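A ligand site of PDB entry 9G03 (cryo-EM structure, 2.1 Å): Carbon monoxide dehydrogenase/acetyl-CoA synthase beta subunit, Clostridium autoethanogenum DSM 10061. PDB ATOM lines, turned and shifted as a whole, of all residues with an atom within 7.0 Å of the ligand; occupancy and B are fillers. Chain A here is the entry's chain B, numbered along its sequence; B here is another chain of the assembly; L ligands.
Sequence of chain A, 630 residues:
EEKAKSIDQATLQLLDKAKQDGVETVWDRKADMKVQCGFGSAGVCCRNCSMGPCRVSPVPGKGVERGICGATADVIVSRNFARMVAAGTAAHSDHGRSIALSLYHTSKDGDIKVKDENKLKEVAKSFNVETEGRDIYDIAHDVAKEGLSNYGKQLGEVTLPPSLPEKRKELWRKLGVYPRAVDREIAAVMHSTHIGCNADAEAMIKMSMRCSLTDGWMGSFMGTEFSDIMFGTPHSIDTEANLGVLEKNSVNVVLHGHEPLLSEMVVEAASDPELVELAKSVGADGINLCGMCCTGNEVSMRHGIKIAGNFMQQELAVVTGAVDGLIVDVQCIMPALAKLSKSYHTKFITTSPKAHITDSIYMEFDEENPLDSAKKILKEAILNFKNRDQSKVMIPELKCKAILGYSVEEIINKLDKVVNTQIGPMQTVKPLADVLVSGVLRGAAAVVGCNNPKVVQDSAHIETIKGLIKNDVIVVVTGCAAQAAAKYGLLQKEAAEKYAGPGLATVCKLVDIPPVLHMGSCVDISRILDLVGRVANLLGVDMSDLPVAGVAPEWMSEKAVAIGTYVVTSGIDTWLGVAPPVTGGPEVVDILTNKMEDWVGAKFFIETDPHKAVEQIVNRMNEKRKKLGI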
ATOM      1  N   CYS A  45      16.951 -17.877  -9.684  1.00  0.00           N
ATOM      2  CA  CYS A  45      16.172 -18.918  -9.034  1.00  0.00           C
ATOM      3  C   CYS A  45      16.393 -20.236  -9.755  1.00  0.00           C
ATOM      4  O   CYS A  45      16.404 -20.283 -10.989  1.00  0.00           O
ATOM      5  CB  CYS A  45      14.682 -18.579  -9.025  1.00  0.00           C
ATOM      6  SG  CYS A  45      13.643 -19.906  -8.374  1.00  0.00           S
ATOM      7  N   CYS A  46      16.534 -21.315  -8.995  1.00  0.00           N
ATOM      8  CA  CYS A  46      16.730 -22.628  -9.567  1.00  0.00           C
ATOM      9  C   CYS A  46      15.735 -23.610  -8.975  1.00  0.00           C
ATOM     10  O   CYS A  46      15.453 -23.585  -7.775  1.00  0.00           O
ATOM     11  CB  CYS A  46      18.152 -23.147  -9.340  1.00  0.00           C
ATOM     12  SG  CYS A  46      18.443 -24.719 -10.150  1.00  0.00           S
ATOM     13  N   ARG A  47      15.203 -24.473  -9.824  1.00  0.00           N
ATOM     14  CA  ARG A  47      14.302 -25.529  -9.396  1.00  0.00           C
ATOM     15  C   ARG A  47      14.653 -26.855 -10.060  1.00  0.00           C
ATOM     16  O   ARG A  47      13.786 -27.711 -10.253  1.00  0.00           O
ATOM     17  CB  ARG A  47      12.843 -25.176  -9.683  1.00  0.00           C
ATOM     18  CG  ARG A  47      12.342 -23.936  -8.965  1.00  0.00           C
ATOM     19  CD  ARG A  47      10.810 -23.822  -9.022  1.00  0.00           C
ATOM     20  NE  ARG A  47      10.314 -23.820 -10.389  1.00  0.00           N
ATOM     21  CZ  ARG A  47      10.012 -22.734 -11.095  1.00  0.00           C
ATOM     22  NH1 ARG A  47      10.095 -21.529 -10.578  1.00  0.00           N
ATOM     23  NH2 ARG A  47       9.605 -22.878 -12.356  1.00  0.00           N
ATOM     24  N   ASN A  48      15.927 -27.033 -10.423  1.00  0.00           N
ATOM     25  CA  ASN A  48      16.333 -28.205 -11.198  1.00  0.00           C
ATOM     26  C   ASN A  48      16.346 -29.496 -10.379  1.00  0.00           C
ATOM     27  O   ASN A  48      16.411 -30.562 -10.981  1.00  0.00           O
ATOM     28  CB  ASN A  48      17.687 -27.947 -11.846  1.00  0.00           C
ATOM     29  CG  ASN A  48      17.607 -26.976 -13.017  1.00  0.00           C
ATOM     30  OD1 ASN A  48      16.633 -26.247 -13.155  1.00  0.00           O
ATOM     31  ND2 ASN A  48      18.633 -26.955 -13.855  1.00  0.00           N
ATOM     32  N   CYS A  49      16.229 -29.431  -9.058  1.00  0.00           N
ATOM     33  CA  CYS A  49      16.119 -30.636  -8.253  1.00  0.00           C
ATOM     34  C   CYS A  49      15.254 -30.350  -7.037  1.00  0.00           C
ATOM     35  O   CYS A  49      15.023 -29.198  -6.687  1.00  0.00           O
ATOM     36  CB  CYS A  49      17.508 -31.170  -7.837  1.00  0.00           C
ATOM     37  SG  CYS A  49      18.271 -30.392  -6.413  1.00  0.00           S
ATOM     38  N   SER A  50      14.793 -31.420  -6.392  1.00  0.00           N
ATOM     39  CA  SER A  50      13.865 -31.268  -5.269  1.00  0.00           C
ATOM     40  C   SER A  50      14.566 -30.951  -3.961  1.00  0.00           C
ATOM     41  O   SER A  50      13.905 -30.842  -2.925  1.00  0.00           O
ATOM     42  CB  SER A  50      12.970 -32.507  -5.114  1.00  0.00           C
ATOM     43  OG  SER A  50      13.687 -33.680  -4.788  1.00  0.00           O
ATOM     44  N   MET A  51      15.903 -30.848  -3.940  1.00  0.00           N
ATOM     45  CA  MET A  51      16.531 -30.171  -2.817  1.00  0.00           C
ATOM     46  C   MET A  51      16.084 -28.715  -2.767  1.00  0.00           C
ATOM     47  O   MET A  51      15.859 -28.170  -1.688  1.00  0.00           O
ATOM     48  CB  MET A  51      18.056 -30.246  -2.914  1.00  0.00           C
ATOM     49  CG  MET A  51      18.633 -31.641  -2.724  1.00  0.00           C
ATOM     50  SD  MET A  51      20.414 -31.664  -2.445  1.00  0.00           S
ATOM     51  CE  MET A  51      21.050 -31.226  -4.060  1.00  0.00           C
ATOM     52  N   GLY A  52      15.910 -28.076  -3.931  1.00  0.00           N
ATOM     53  CA  GLY A  52      15.398 -26.730  -4.008  1.00  0.00           C
ATOM     54  C   GLY A  52      13.926 -26.615  -3.676  1.00  0.00           C
ATOM     55  O   GLY A  52      13.316 -27.546  -3.149  1.00  0.00           O
ATOM     56  N   PRO A  53      13.294 -25.484  -4.036  1.00  0.00           N
ATOM     57  CA  PRO A  53      13.830 -24.368  -4.843  1.00  0.00           C
ATOM     58  C   PRO A  53      14.936 -23.553  -4.163  1.00  0.00           C
ATOM     59  O   PRO A  53      14.875 -23.288  -2.977  1.00  0.00           O
ATOM     60  CB  PRO A  53      12.584 -23.476  -5.062  1.00  0.00           C
ATOM     61  CG  PRO A  53      11.390 -24.306  -4.640  1.00  0.00           C
ATOM     62  CD  PRO A  53      11.915 -25.235  -3.601  1.00  0.00           C
ATOM     63  N   CYS A  54      15.928 -23.122  -4.938  1.00  0.00           N
ATOM     64  CA  CYS A  54      17.028 -22.301  -4.449  1.00  0.00           C
ATOM     65  C   CYS A  54      17.011 -20.953  -5.143  1.00  0.00           C
ATOM     66  O   CYS A  54      16.860 -20.888  -6.370  1.00  0.00           O
ATOM     67  CB  CYS A  54      18.399 -22.970  -4.658  1.00  0.00           C
ATOM     68  SG  CYS A  54      18.687 -24.553  -3.798  1.00  0.00           S
ATOM     69  N   ARG A  55      17.159 -19.889  -4.372  1.00  0.00           N
ATOM     70  CA  ARG A  55      17.328 -18.550  -4.912  1.00  0.00           C
ATOM     71  C   ARG A  55      18.575 -17.950  -4.291  1.00  0.00           C
ATOM     72  O   ARG A  55      18.766 -18.004  -3.075  1.00  0.00           O
ATOM     73  CB  ARG A  55      16.099 -17.672  -4.676  1.00  0.00           C
ATOM     74  CG  ARG A  55      15.499 -17.754  -3.305  1.00  0.00           C
ATOM     75  CD  ARG A  55      14.125 -17.139  -3.279  1.00  0.00           C
ATOM     76  NE  ARG A  55      13.550 -17.227  -1.950  1.00  0.00           N
ATOM     77  CZ  ARG A  55      12.280 -16.999  -1.653  1.00  0.00           C
ATOM     78  NH1 ARG A  55      11.407 -16.663  -2.581  1.00  0.00           N
ATOM     79  NH2 ARG A  55      11.885 -17.125  -0.387  1.00  0.00           N
ATOM     80  N   VAL A  56      19.445 -17.420  -5.144  1.00  0.00           N
ATOM     81  CA  VAL A  56      20.653 -16.765  -4.713  1.00  0.00           C
ATOM     82  C   VAL A  56      20.533 -15.287  -5.053  1.00  0.00           C
ATOM     83  O   VAL A  56      19.740 -14.885  -5.906  1.00  0.00           O
ATOM     84  CB  VAL A  56      21.907 -17.396  -5.359  1.00  0.00           C
ATOM     85  CG1 VAL A  56      22.042 -18.849  -4.902  1.00  0.00           C
ATOM     86  CG2 VAL A  56      21.828 -17.313  -6.886  1.00  0.00           C
ATOM     87  N   ARG A  66      25.135 -19.339  -2.876  1.00  0.00           N
ATOM     88  CA  ARG A  66      25.072 -20.597  -3.595  1.00  0.00           C
ATOM     89  C   ARG A  66      23.789 -21.324  -3.283  1.00  0.00           C
ATOM     90  O   ARG A  66      23.236 -21.214  -2.191  1.00  0.00           O
ATOM     91  CB  ARG A  66      26.275 -21.488  -3.243  1.00  0.00           C
ATOM     92  CG  ARG A  66      27.621 -20.899  -3.649  1.00  0.00           C
ATOM     93  CD  ARG A  66      28.792 -21.723  -3.108  1.00  0.00           C
ATOM     94  NE  ARG A  66      30.066 -21.295  -3.667  1.00  0.00           N
ATOM     95  CZ  ARG A  66      30.709 -21.886  -4.668  1.00  0.00           C
ATOM     96  NH1 ARG A  66      30.245 -22.993  -5.242  1.00  0.00           N
ATOM     97  NH2 ARG A  66      31.858 -21.374  -5.092  1.00  0.00           N
ATOM     98  N   GLY A  67      23.330 -22.109  -4.255  1.00  0.00           N
ATOM     99  CA  GLY A  67      22.260 -23.048  -4.013  1.00  0.00           C
ATOM    100  C   GLY A  67      22.722 -24.146  -3.078  1.00  0.00           C
ATOM    101  O   GLY A  67      23.891 -24.237  -2.694  1.00  0.00           O
ATOM    102  N   ILE A  68      21.791 -25.041  -2.766  1.00  0.00           N
ATOM    103  CA  ILE A  68      22.051 -26.092  -1.783  1.00  0.00           C
ATOM    104  C   ILE A  68      23.157 -27.020  -2.265  1.00  0.00           C
ATOM    105  O   ILE A  68      24.045 -27.399  -1.497  1.00  0.00           O
ATOM    106  CB  ILE A  68      20.748 -26.834  -1.438  1.00  0.00           C
ATOM    107  CG1 ILE A  68      19.790 -25.879  -0.709  1.00  0.00           C
ATOM    108  CG2 ILE A  68      21.051 -28.063  -0.560  1.00  0.00           C
ATOM    109  CD1 ILE A  68      18.379 -26.380  -0.528  1.00  0.00           C
ATOM    110  N   CYS A  69      23.152 -27.352  -3.561  1.00  0.00           N
ATOM    111  CA  CYS A  69      24.209 -28.167  -4.164  1.00  0.00           C
ATOM    112  C   CYS A  69      25.534 -27.420  -4.294  1.00  0.00           C
ATOM    113  O   CYS A  69      26.542 -28.031  -4.655  1.00  0.00           O
ATOM    114  CB  CYS A  69      23.765 -28.662  -5.544  1.00  0.00           C
ATOM    115  SG  CYS A  69      23.645 -27.373  -6.804  1.00  0.00           S
ATOM    116  N   GLY A  70      25.542 -26.112  -4.044  1.00  0.00           N
ATOM    117  CA  GLY A  70      26.711 -25.271  -4.203  1.00  0.00           C
ATOM    118  C   GLY A  70      26.800 -24.483  -5.494  1.00  0.00           C
ATOM    119  O   GLY A  70      27.800 -23.812  -5.707  1.00  0.00           O
ATOM    120  N   ALA A  71      25.774 -24.521  -6.329  1.00  0.00           N
ATOM    121  CA  ALA A  71      25.794 -23.796  -7.601  1.00  0.00           C
ATOM    122  C   ALA A  71      25.732 -22.276  -7.400  1.00  0.00           C
ATOM    123  O   ALA A  71      24.904 -21.772  -6.646  1.00  0.00           O
ATOM    124  CB  ALA A  71      24.616 -24.258  -8.461  1.00  0.00           C
ATOM    125  N   THR A  72      26.606 -21.558  -8.101  1.00  0.00           N
ATOM    126  CA  THR A  72      26.674 -20.106  -8.019  1.00  0.00           C
ATOM    127  C   THR A  72      25.570 -19.456  -8.848  1.00  0.00           C
ATOM    128  O   THR A  72      24.866 -20.113  -9.610  1.00  0.00           O
ATOM    129  CB  THR A  72      28.024 -19.590  -8.508  1.00  0.00           C
ATOM    130  OG1 THR A  72      28.212 -20.015  -9.871  1.00  0.00           O
ATOM    131  CG2 THR A  72      29.158 -20.118  -7.653  1.00  0.00           C
ATOM    132  N   ILE A  76      23.481 -20.976 -12.126  1.00  0.00           N
ATOM    133  CA  ILE A  76      22.021 -21.027 -12.185  1.00  0.00           C
ATOM    134  C   ILE A  76      21.509 -20.257 -13.408  1.00  0.00           C
ATOM    135  O   ILE A  76      20.660 -20.746 -14.165  1.00  0.00           O
ATOM    136  CB  ILE A  76      21.419 -20.500 -10.868  1.00  0.00           C
ATOM    137  CG1 ILE A  76      21.849 -21.425  -9.699  1.00  0.00           C
ATOM    138  CG2 ILE A  76      19.880 -20.357 -10.936  1.00  0.00           C
ATOM    139  CD1 ILE A  76      21.545 -20.907  -8.328  1.00  0.00           C
ATOM    140  N   ARG A  79      22.430 -22.190 -16.728  1.00  0.00           N
ATOM    141  CA  ARG A  79      21.569 -23.356 -16.955  1.00  0.00           C
ATOM    142  C   ARG A  79      20.168 -22.943 -17.368  1.00  0.00           C
ATOM    143  O   ARG A  79      19.611 -23.505 -18.313  1.00  0.00           O
ATOM    144  CB  ARG A  79      21.539 -24.244 -15.698  1.00  0.00           C
ATOM    145  CG  ARG A  79      22.890 -24.882 -15.393  1.00  0.00           C
ATOM    146  CD  ARG A  79      22.822 -25.936 -14.302  1.00  0.00           C
ATOM    147  NE  ARG A  79      22.280 -25.425 -13.046  1.00  0.00           N
ATOM    148  CZ  ARG A  79      22.328 -26.088 -11.900  1.00  0.00           C
ATOM    149  NH1 ARG A  79      22.947 -27.248 -11.800  1.00  0.00           N
ATOM    150  NH2 ARG A  79      21.718 -25.574 -10.826  1.00  0.00           N
ATOM    151  N   THR A 193      22.300 -29.606 -17.864  1.00  0.00           N
ATOM    152  CA  THR A 193      21.685 -28.761 -16.840  1.00  0.00           C
ATOM    153  C   THR A 193      21.190 -29.551 -15.624  1.00  0.00           C
ATOM    154  O   THR A 193      20.758 -28.926 -14.657  1.00  0.00           O
ATOM    155  CB  THR A 193      20.535 -27.955 -17.452  1.00  0.00           C
ATOM    156  OG1 THR A 193      19.580 -28.826 -18.043  1.00  0.00           O
ATOM    157  CG2 THR A 193      21.044 -26.982 -18.508  1.00  0.00           C
ATOM    158  N   HIS A 194      21.231 -30.876 -15.660  1.00  0.00           N
ATOM    159  CA  HIS A 194      20.788 -31.685 -14.521  1.00  0.00           C
ATOM    160  C   HIS A 194      21.661 -31.414 -13.284  1.00  0.00           C
ATOM    161  O   HIS A 194      22.836 -31.064 -13.408  1.00  0.00           O
ATOM    162  CB  HIS A 194      20.866 -33.174 -14.889  1.00  0.00           C
ATOM    163  CG  HIS A 194      20.343 -34.092 -13.828  1.00  0.00           C
ATOM    164  ND1 HIS A 194      21.109 -34.502 -12.764  1.00  0.00           N
ATOM    165  CD2 HIS A 194      19.152 -34.710 -13.700  1.00  0.00           C
ATOM    166  CE1 HIS A 194      20.399 -35.314 -12.005  1.00  0.00           C
ATOM    167  NE2 HIS A 194      19.209 -35.459 -12.546  1.00  0.00           N
ATOM    168  N   ILE A 195      21.077 -31.582 -12.104  1.00  0.00           N
ATOM    169  CA  ILE A 195      21.795 -31.270 -10.866  1.00  0.00           C
ATOM    170  C   ILE A 195      23.135 -32.005 -10.869  1.00  0.00           C
ATOM    171  O   ILE A 195      23.210 -33.188 -11.239  1.00  0.00           O
ATOM    172  CB  ILE A 195      20.946 -31.640  -9.621  1.00  0.00           C
ATOM    173  CG1 ILE A 195      21.759 -31.645  -8.334  1.00  0.00           C
ATOM    174  CG2 ILE A 195      20.346 -33.028  -9.723  1.00  0.00           C
ATOM    175  CD1 ILE A 195      22.287 -30.363  -7.926  1.00  0.00           C
ATOM    176  N   GLY A 196      24.194 -31.301 -10.535  1.00  0.00           N
ATOM    177  CA  GLY A 196      25.494 -31.924 -10.403  1.00  0.00           C
ATOM    178  C   GLY A 196      26.156 -32.321 -11.705  1.00  0.00           C
ATOM    179  O   GLY A 196      26.996 -33.212 -11.710  1.00  0.00           O
ATOM    180  N   MET B  33      19.537 -21.447   3.064  1.00  0.00           N
ATOM    181  CA  MET B  33      18.398 -21.191   2.205  1.00  0.00           C
ATOM    182  C   MET B  33      17.141 -20.887   3.000  1.00  0.00           C
ATOM    183  O   MET B  33      16.203 -20.295   2.453  1.00  0.00           O
ATOM    184  CB  MET B  33      18.184 -22.392   1.275  1.00  0.00           C
ATOM    185  CG  MET B  33      17.412 -22.066   0.026  1.00  0.00           C
ATOM    186  SD  MET B  33      18.135 -20.756  -0.995  1.00  0.00           S
ATOM    187  CE  MET B  33      19.676 -21.506  -1.513  1.00  0.00           C
ATOM    188  N   GLN B  36      12.119 -22.047   1.968  1.00  0.00           N
ATOM    189  CA  GLN B  36      12.172 -22.023   0.516  1.00  0.00           C
ATOM    190  C   GLN B  36      10.859 -21.488  -0.066  1.00  0.00           C
ATOM    191  O   GLN B  36       9.798 -21.581   0.543  1.00  0.00           O
ATOM    192  CB  GLN B  36      12.498 -23.408  -0.027  1.00  0.00           C
ATOM    193  CG  GLN B  36      13.911 -23.842   0.300  1.00  0.00           C
ATOM    194  CD  GLN B  36      14.193 -25.252  -0.141  1.00  0.00           C
ATOM    195  OE1 GLN B  36      13.510 -26.186   0.276  1.00  0.00           O
ATOM    196  NE2 GLN B  36      15.168 -25.432  -1.013  1.00  0.00           N
ATOM    197  N   PRO B 335      28.793 -29.038  -7.214  1.00  0.00           N
ATOM    198  CA  PRO B 335      29.854 -28.089  -7.627  1.00  0.00           C
ATOM    199  C   PRO B 335      30.629 -27.525  -6.448  1.00  0.00           C
ATOM    200  O   PRO B 335      31.815 -27.213  -6.604  1.00  0.00           O
ATOM    201  CB  PRO B 335      29.073 -27.010  -8.398  1.00  0.00           C
ATOM    202  CG  PRO B 335      27.661 -27.153  -8.022  1.00  0.00           C
ATOM    203  CD  PRO B 335      27.466 -28.609  -7.685  1.00  0.00           C
ATOM    204  N   MET B 556      16.023 -36.783  -4.767  1.00  0.00           N
ATOM    205  CA  MET B 556      16.242 -35.363  -5.027  1.00  0.00           C
ATOM    206  C   MET B 556      16.312 -35.019  -6.514  1.00  0.00           C
ATOM    207  O   MET B 556      15.946 -33.907  -6.901  1.00  0.00           O
ATOM    208  CB  MET B 556      17.521 -34.887  -4.308  1.00  0.00           C
ATOM    209  CG  MET B 556      18.823 -35.400  -4.891  1.00  0.00           C
ATOM    210  SD  MET B 556      19.593 -34.395  -6.192  1.00  0.00           S
ATOM    211  CE  MET B 556      20.918 -35.493  -6.683  1.00  0.00           C
HETATM  212 FE1  LIG L   1      19.240 -25.848  -5.598  1.00  0.00          FE
HETATM  213 FE2  LIG L   1      21.381 -26.950  -6.928  1.00  0.00          FE
HETATM  214 FE3  LIG L   1      19.267 -25.906  -8.347  1.00  0.00          FE
HETATM  215 FE4  LIG L   1      18.959 -28.236  -6.921  1.00  0.00          FE
HETATM  216  S1  LIG L   1      20.317 -27.894  -8.727  1.00  0.00           S
HETATM  217  S2  LIG L   1      17.522 -26.461  -6.967  1.00  0.00           S
HETATM  218  S3  LIG L   1      20.296 -27.816  -5.115  1.00  0.00           S
HETATM  219  S4  LIG L   1      20.711 -24.769  -6.970  1.00  0.00           S
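The backbone carbonyl oxygen (O) of Cys 54 is in hydrogen-bond range of the backbone NH (N) of Cys 46.
N of Ile 68 lies close to SG of Cys 54.
N of Ala 71 sits close to SG of Cys 69 (3.6 Å).
NH2 of Arg 79 sits close to SG of Cys 46 (3.5 Å).
The side-chain sulfur (SG) of Cys 46 sits close to the backbone NH (N) of Asn 48 (3.4 Å).
N of Met 51 lies close to SG of Cys 49 (3.5 Å).
The backbone carbonyl oxygen (O) of Met 51 sits at hydrogen-bond distance from the side-chain amide nitrogen (NE2) of Gln 36 of chain B, 2.9 Å away.
The backbone carbonyl oxygen (O) of Thr 193 lies within hydrogen-bond range of the side-chain amide nitrogen (ND2) of Asn 48 (3.0 Å).
Residues that only touch the ligand: Ile 195, Met 51, Gly 67, Ile 68 and Asn 48.
11 residues have an atom within 4 Å of the ligand: Cys 46, Asn 48, Cys 49, Met 51, Gly 52, Cys 54, Gly 67, Ile 68, Cys 69, Arg 79 and Ile 195.
The nearest printed residue that does not touch the ligand is Arg 47 (4.1 Å).
An iron atom (FE1) of the ligand is bound by the side-chain sulfur (SG) of Cys 54 (2.3 Å).
N of Cys 69 lies close to S3 of the ligand (3.3 Å).
SG of Cys 69 binds FE2 of the ligand (2.3 Å).
FE3 of the ligand is bound by SG of Cys 46, at 2.3 Å.
An iron atom (FE4) of the ligand is bound by the side-chain sulfur of Cys 49, 2.3 Å away.
A sulfur (S1) of the ligand sits close to the guanidinium group (NH2) of Arg 79, 3.4 Å away.
A sulfur (S2) of the ligand lies close to the backbone NH (N) of Gly 52.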
